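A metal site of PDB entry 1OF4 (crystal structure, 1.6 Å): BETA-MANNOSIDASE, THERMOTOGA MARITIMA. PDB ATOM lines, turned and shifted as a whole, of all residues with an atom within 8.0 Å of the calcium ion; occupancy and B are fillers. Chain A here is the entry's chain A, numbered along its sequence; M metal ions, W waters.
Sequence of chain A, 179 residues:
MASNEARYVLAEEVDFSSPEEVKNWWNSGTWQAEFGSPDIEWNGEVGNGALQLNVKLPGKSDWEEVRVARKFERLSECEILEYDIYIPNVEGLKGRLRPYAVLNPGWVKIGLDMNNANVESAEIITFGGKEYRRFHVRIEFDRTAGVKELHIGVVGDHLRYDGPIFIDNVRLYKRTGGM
Four residues have an atom within 4 Å of the calcium ion: Asp 15, Gly 47, Gly 49 and Asp 168. The nearest printed residue that does not touch the calcium ion is Asn 48 (4.2 Å).
Water W1 bridges the backbone carbonyl oxygen of Asn 48 (2.9 Å) and the side-chain hydroxyl of Ser 17 (3.1 Å).
The side-chain amide oxygen (OD1) of Asn 169 lies close to the side-chain carboxylate (OD1) of Asp 15 (3.4 Å).
The calcium ion is bound by O of Gly 49 (2.3 Å). O of Asp 15 binds the calcium ion, at 2.3 Å. Water W1 binds the calcium ion. Water W2 is bound to the calcium ion (2.4 Å). O of Gly 47 is bound to the calcium ion, at 2.4 Å. The calcium ion is bound by OD2 of Asp 168 (2.5 Å). The side-chain carboxylate (OD1) of Asp 168 is bound to the calcium ion (2.5 Å). The calcium ion has seven donor atoms within binding distance.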
ATOM      1  N   VAL A  14     -24.655  26.614  13.991  1.00  0.00           N
ATOM      2  CA  VAL A  14     -24.684  25.172  14.143  1.00  0.00           C
ATOM      3  C   VAL A  14     -23.409  24.620  13.535  1.00  0.00           C
ATOM      4  O   VAL A  14     -23.196  24.712  12.337  1.00  0.00           O
ATOM      5  CB  VAL A  14     -25.917  24.536  13.482  1.00  0.00           C
ATOM      6  CG1 VAL A  14     -25.810  23.061  13.628  1.00  0.00           C
ATOM      7  CG2 VAL A  14     -27.198  25.032  14.167  1.00  0.00           C
ATOM      8  N   ASP A  15     -22.579  24.049  14.372  1.00  0.00           N
ATOM      9  CA  ASP A  15     -21.323  23.407  13.956  1.00  0.00           C
ATOM     10  C   ASP A  15     -21.367  21.894  13.999  1.00  0.00           C
ATOM     11  O   ASP A  15     -20.357  21.248  13.650  1.00  0.00           O
ATOM     12  CB  ASP A  15     -20.142  23.913  14.805  1.00  0.00           C
ATOM     13  CG  ASP A  15     -19.912  25.347  14.630  1.00  0.00           C
ATOM     14  OD1 ASP A  15     -20.142  25.878  13.521  1.00  0.00           O
ATOM     15  OD2 ASP A  15     -19.565  26.084  15.579  1.00  0.00           O
ATOM     16  N   PHE A  16     -22.474  21.312  14.466  1.00  0.00           N
ATOM     17  CA  PHE A  16     -22.668  19.860  14.501  1.00  0.00           C
ATOM     18  C   PHE A  16     -21.562  19.183  15.314  1.00  0.00           C
ATOM     19  O   PHE A  16     -21.090  18.120  14.970  1.00  0.00           O
ATOM     20  CB  PHE A  16     -22.750  19.271  13.091  1.00  0.00           C
ATOM     21  CG  PHE A  16     -23.806  19.878  12.216  1.00  0.00           C
ATOM     22  CD1 PHE A  16     -25.125  19.488  12.311  1.00  0.00           C
ATOM     23  CD2 PHE A  16     -23.473  20.869  11.329  1.00  0.00           C
ATOM     24  CE1 PHE A  16     -26.080  20.095  11.501  1.00  0.00           C
ATOM     25  CE2 PHE A  16     -24.407  21.445  10.521  1.00  0.00           C
ATOM     26  CZ  PHE A  16     -25.729  21.029  10.598  1.00  0.00           C
ATOM     27  N   SER A  17     -21.143  19.823  16.405  1.00  0.00           N
ATOM     28  CA  SER A  17     -20.087  19.263  17.260  1.00  0.00           C
ATOM     29  C   SER A  17     -20.473  17.975  17.942  1.00  0.00           C
ATOM     30  O   SER A  17     -19.623  17.131  18.271  1.00  0.00           O
ATOM     31  CB  SER A  17     -19.591  20.322  18.244  1.00  0.00           C
ATOM     32  OG  SER A  17     -18.608  21.088  17.562  1.00  0.00           O
ATOM     33  N   SER A  18     -21.767  17.762  18.067  1.00  0.00           N
ATOM     34  CA  SER A  18     -22.293  16.585  18.700  1.00  0.00           C
ATOM     35  C   SER A  18     -23.408  15.955  17.891  1.00  0.00           C
ATOM     36  O   SER A  18     -24.204  16.651  17.264  1.00  0.00           O
ATOM     37  CB  SER A  18     -22.793  16.918  20.122  1.00  0.00           C
ATOM     38  OG  SER A  18     -23.750  15.945  20.556  1.00  0.00           O
ATOM     39  N   TRP A  42     -25.159  11.936  11.644  1.00  0.00           N
ATOM     40  CA  TRP A  42     -23.956  12.601  12.073  1.00  0.00           C
ATOM     41  C   TRP A  42     -22.696  11.923  11.555  1.00  0.00           C
ATOM     42  O   TRP A  42     -22.621  10.680  11.462  1.00  0.00           O
ATOM     43  CB  TRP A  42     -23.906  12.644  13.605  1.00  0.00           C
ATOM     44  CG  TRP A  42     -22.849  13.541  14.184  1.00  0.00           C
ATOM     45  CD1 TRP A  42     -22.814  14.905  14.152  1.00  0.00           C
ATOM     46  CD2 TRP A  42     -21.707  13.127  14.920  1.00  0.00           C
ATOM     47  NE1 TRP A  42     -21.697  15.373  14.811  1.00  0.00           N
ATOM     48  CE2 TRP A  42     -21.000  14.297  15.298  1.00  0.00           C
ATOM     49  CE3 TRP A  42     -21.177  11.881  15.284  1.00  0.00           C
ATOM     50  CZ2 TRP A  42     -19.816  14.243  16.040  1.00  0.00           C
ATOM     51  CZ3 TRP A  42     -20.012  11.849  16.018  1.00  0.00           C
ATOM     52  CH2 TRP A  42     -19.348  13.010  16.394  1.00  0.00           C
ATOM     53  N   ASN A  43     -21.706  12.750  11.248  1.00  0.00           N
ATOM     54  CA  ASN A  43     -20.353  12.295  10.918  1.00  0.00           C
ATOM     55  C   ASN A  43     -19.373  13.047  11.806  1.00  0.00           C
ATOM     56  O   ASN A  43     -19.343  14.258  11.772  1.00  0.00           O
ATOM     57  CB  ASN A  43     -20.038  12.482   9.429  1.00  0.00           C
ATOM     58  CG  ASN A  43     -18.745  11.817   9.028  1.00  0.00           C
ATOM     59  OD1 ASN A  43     -17.680  12.182   9.536  1.00  0.00           O
ATOM     60  ND2 ASN A  43     -18.819  10.798   8.118  1.00  0.00           N
ATOM     61  N   GLY A  44     -18.582  12.304  12.598  1.00  0.00           N
ATOM     62  CA  GLY A  44     -17.634  12.946  13.499  1.00  0.00           C
ATOM     63  C   GLY A  44     -16.241  13.210  12.973  1.00  0.00           C
ATOM     64  O   GLY A  44     -15.439  13.814  13.668  1.00  0.00           O
ATOM     65  N   GLU A  45     -15.908  12.747  11.770  1.00  0.00           N
ATOM     66  CA  GLU A  45     -14.582  13.099  11.204  1.00  0.00           C
ATOM     67  C   GLU A  45     -14.647  14.394  10.374  1.00  0.00           C
ATOM     68  O   GLU A  45     -13.878  15.376  10.549  1.00  0.00           O
ATOM     69  CB  GLU A  45     -14.003  11.976  10.345  1.00  0.00           C
ATOM     70  CG  GLU A  45     -13.979  10.563  10.888  1.00  0.00           C
ATOM     71  CD  GLU A  45     -13.628   9.538   9.796  1.00  0.00           C
ATOM     72  OE1 GLU A  45     -12.947   9.937   8.799  1.00  0.00           O
ATOM     73  OE2 GLU A  45     -14.042   8.341   9.907  1.00  0.00           O
ATOM     74  N   VAL A  46     -15.615  14.442   9.489  1.00  0.00           N
ATOM     75  CA  VAL A  46     -15.689  15.580   8.600  1.00  0.00           C
ATOM     76  C   VAL A  46     -16.082  16.811   9.430  1.00  0.00           C
ATOM     77  O   VAL A  46     -17.026  16.751  10.209  1.00  0.00           O
ATOM     78  CB  VAL A  46     -16.702  15.317   7.517  1.00  0.00           C
ATOM     79  CG1 VAL A  46     -16.885  16.557   6.629  1.00  0.00           C
ATOM     80  CG2 VAL A  46     -16.259  14.136   6.681  1.00  0.00           C
ATOM     81  N   GLY A  47     -15.310  17.879   9.309  1.00  0.00           N
ATOM     82  CA  GLY A  47     -15.632  19.153   9.928  1.00  0.00           C
ATOM     83  C   GLY A  47     -15.636  19.129  11.452  1.00  0.00           C
ATOM     84  O   GLY A  47     -16.272  19.963  12.069  1.00  0.00           O
ATOM     85  N   ASN A  48     -14.906  18.193  12.039  1.00  0.00           N
ATOM     86  CA  ASN A  48     -15.019  17.830  13.471  1.00  0.00           C
ATOM     87  C   ASN A  48     -16.457  17.683  13.937  1.00  0.00           C
ATOM     88  O   ASN A  48     -16.808  18.128  15.038  1.00  0.00           O
ATOM     89  CB  ASN A  48     -14.270  18.754  14.452  1.00  0.00           C
ATOM     90  CG  ASN A  48     -13.722  19.992  13.845  1.00  0.00           C
ATOM     91  OD1 ASN A  48     -12.617  19.999  13.231  1.00  0.00           O
ATOM     92  ND2 ASN A  48     -14.419  21.106  14.083  1.00  0.00           N
ATOM     93  N   GLY A  49     -17.261  17.015  13.104  1.00  0.00           N
ATOM     94  CA  GLY A  49     -18.689  16.914  13.303  1.00  0.00           C
ATOM     95  C   GLY A  49     -19.383  17.690  12.202  1.00  0.00           C
ATOM     96  O   GLY A  49     -19.196  18.887  12.055  1.00  0.00           O
ATOM     97  N   ALA A  50     -20.182  16.992  11.404  1.00  0.00           N
ATOM     98  CA  ALA A  50     -20.903  17.577  10.277  1.00  0.00           C
ATOM     99  C   ALA A  50     -22.162  16.743  10.019  1.00  0.00           C
ATOM    100  O   ALA A  50     -22.314  15.633  10.508  1.00  0.00           O
ATOM    101  CB  ALA A  50     -20.037  17.627   9.042  1.00  0.00           C
ATOM    102  N   LEU A  51     -23.112  17.361   9.337  1.00  0.00           N
ATOM    103  CA  LEU A  51     -24.332  16.708   8.921  1.00  0.00           C
ATOM    104  C   LEU A  51     -24.072  15.976   7.601  1.00  0.00           C
ATOM    105  O   LEU A  51     -23.726  16.614   6.597  1.00  0.00           O
ATOM    106  CB  LEU A  51     -25.425  17.739   8.714  1.00  0.00           C
ATOM    107  CG  LEU A  51     -26.858  17.238   8.582  1.00  0.00           C
ATOM    108  CD1 LEU A  51     -27.431  16.545   9.815  1.00  0.00           C
ATOM    109  CD2 LEU A  51     -27.834  18.382   8.143  1.00  0.00           C
ATOM    110  N   TYR A  86     -19.332  20.082   1.828  1.00  0.00           N
ATOM    111  CA  TYR A  86     -18.159  19.276   1.480  1.00  0.00           C
ATOM    112  C   TYR A  86     -18.597  18.041   0.709  1.00  0.00           C
ATOM    113  O   TYR A  86     -19.563  17.401   1.091  1.00  0.00           O
ATOM    114  CB  TYR A  86     -17.424  18.841   2.745  1.00  0.00           C
ATOM    115  CG  TYR A  86     -17.061  19.972   3.709  1.00  0.00           C
ATOM    116  CD1 TYR A  86     -16.411  21.115   3.274  1.00  0.00           C
ATOM    117  CD2 TYR A  86     -17.348  19.861   5.054  1.00  0.00           C
ATOM    118  CE1 TYR A  86     -16.075  22.115   4.148  1.00  0.00           C
ATOM    119  CE2 TYR A  86     -16.994  20.860   5.937  1.00  0.00           C
ATOM    120  CZ  TYR A  86     -16.367  21.988   5.479  1.00  0.00           C
ATOM    121  OH  TYR A  86     -16.001  23.025   6.341  1.00  0.00           O
ATOM    122  N   PHE A 127      -9.785  16.537   5.976  1.00  0.00           N
ATOM    123  CA  PHE A 127     -10.164  15.994   7.279  1.00  0.00           C
ATOM    124  C   PHE A 127      -9.740  14.536   7.324  1.00  0.00           C
ATOM    125  O   PHE A 127     -10.126  13.744   6.475  1.00  0.00           O
ATOM    126  CB  PHE A 127     -11.691  16.053   7.485  1.00  0.00           C
ATOM    127  CG  PHE A 127     -12.255  17.414   7.446  1.00  0.00           C
ATOM    128  CD1 PHE A 127     -11.933  18.347   8.412  1.00  0.00           C
ATOM    129  CD2 PHE A 127     -13.111  17.790   6.423  1.00  0.00           C
ATOM    130  CE1 PHE A 127     -12.461  19.628   8.364  1.00  0.00           C
ATOM    131  CE2 PHE A 127     -13.649  19.060   6.348  1.00  0.00           C
ATOM    132  CZ  PHE A 127     -13.302  20.001   7.332  1.00  0.00           C
ATOM    133  N   ILE A 167     -22.847  19.027   5.256  1.00  0.00           N
ATOM    134  CA  ILE A 167     -23.125  20.414   5.567  1.00  0.00           C
ATOM    135  C   ILE A 167     -22.483  20.757   6.910  1.00  0.00           C
ATOM    136  O   ILE A 167     -22.446  19.934   7.826  1.00  0.00           O
ATOM    137  CB  ILE A 167     -24.688  20.616   5.629  1.00  0.00           C
ATOM    138  CG1 ILE A 167     -25.305  20.469   4.222  1.00  0.00           C
ATOM    139  CG2 ILE A 167     -25.012  21.970   6.210  1.00  0.00           C
ATOM    140  CD1 ILE A 167     -26.841  20.241   4.226  1.00  0.00           C
ATOM    141  N   ASP A 168     -21.916  21.932   7.008  1.00  0.00           N
ATOM    142  CA  ASP A 168     -21.306  22.363   8.263  1.00  0.00           C
ATOM    143  C   ASP A 168     -21.364  23.886   8.386  1.00  0.00           C
ATOM    144  O   ASP A 168     -21.655  24.585   7.412  1.00  0.00           O
ATOM    145  CB  ASP A 168     -19.869  21.858   8.350  1.00  0.00           C
ATOM    146  CG  ASP A 168     -19.342  21.710   9.784  1.00  0.00           C
ATOM    147  OD1 ASP A 168     -20.058  21.960  10.801  1.00  0.00           O
ATOM    148  OD2 ASP A 168     -18.194  21.306   9.964  1.00  0.00           O
ATOM    149  N   ASN A 169     -21.120  24.392   9.597  1.00  0.00           N
ATOM    150  CA  ASN A 169     -20.894  25.815   9.836  1.00  0.00           C
ATOM    151  C   ASN A 169     -22.073  26.670   9.385  1.00  0.00           C
ATOM    152  O   ASN A 169     -21.914  27.651   8.691  1.00  0.00           O
ATOM    153  CB  ASN A 169     -19.585  26.252   9.174  1.00  0.00           C
ATOM    154  CG  ASN A 169     -18.431  25.411   9.610  1.00  0.00           C
ATOM    155  OD1 ASN A 169     -18.282  25.127  10.808  1.00  0.00           O
ATOM    156  ND2 ASN A 169     -17.580  24.988   8.648  1.00  0.00           N
ATOM    157  N   VAL A 170     -23.267  26.276   9.792  1.00  0.00           N
ATOM    158  CA  VAL A 170     -24.466  27.021   9.465  1.00  0.00           C
ATOM    159  C   VAL A 170     -24.516  28.227  10.388  1.00  0.00           C
ATOM    160  O   VAL A 170     -24.579  28.051  11.592  1.00  0.00           O
ATOM    161  CB  VAL A 170     -25.731  26.127   9.624  1.00  0.00           C
ATOM    162  CG1 VAL A 170     -26.973  26.919   9.321  1.00  0.00           C
ATOM    163  CG2 VAL A 170     -25.659  24.951   8.681  1.00  0.00           C
HETATM  164 CA    CA M   1     -18.397  21.050  12.398  1.00  0.00          CA
HETATM  165  O   HOH W   1     -17.620  20.909  14.638  1.00  0.00           O
HETATM  166  O   HOH W   2     -17.495  23.249  12.490  1.00  0.00           O
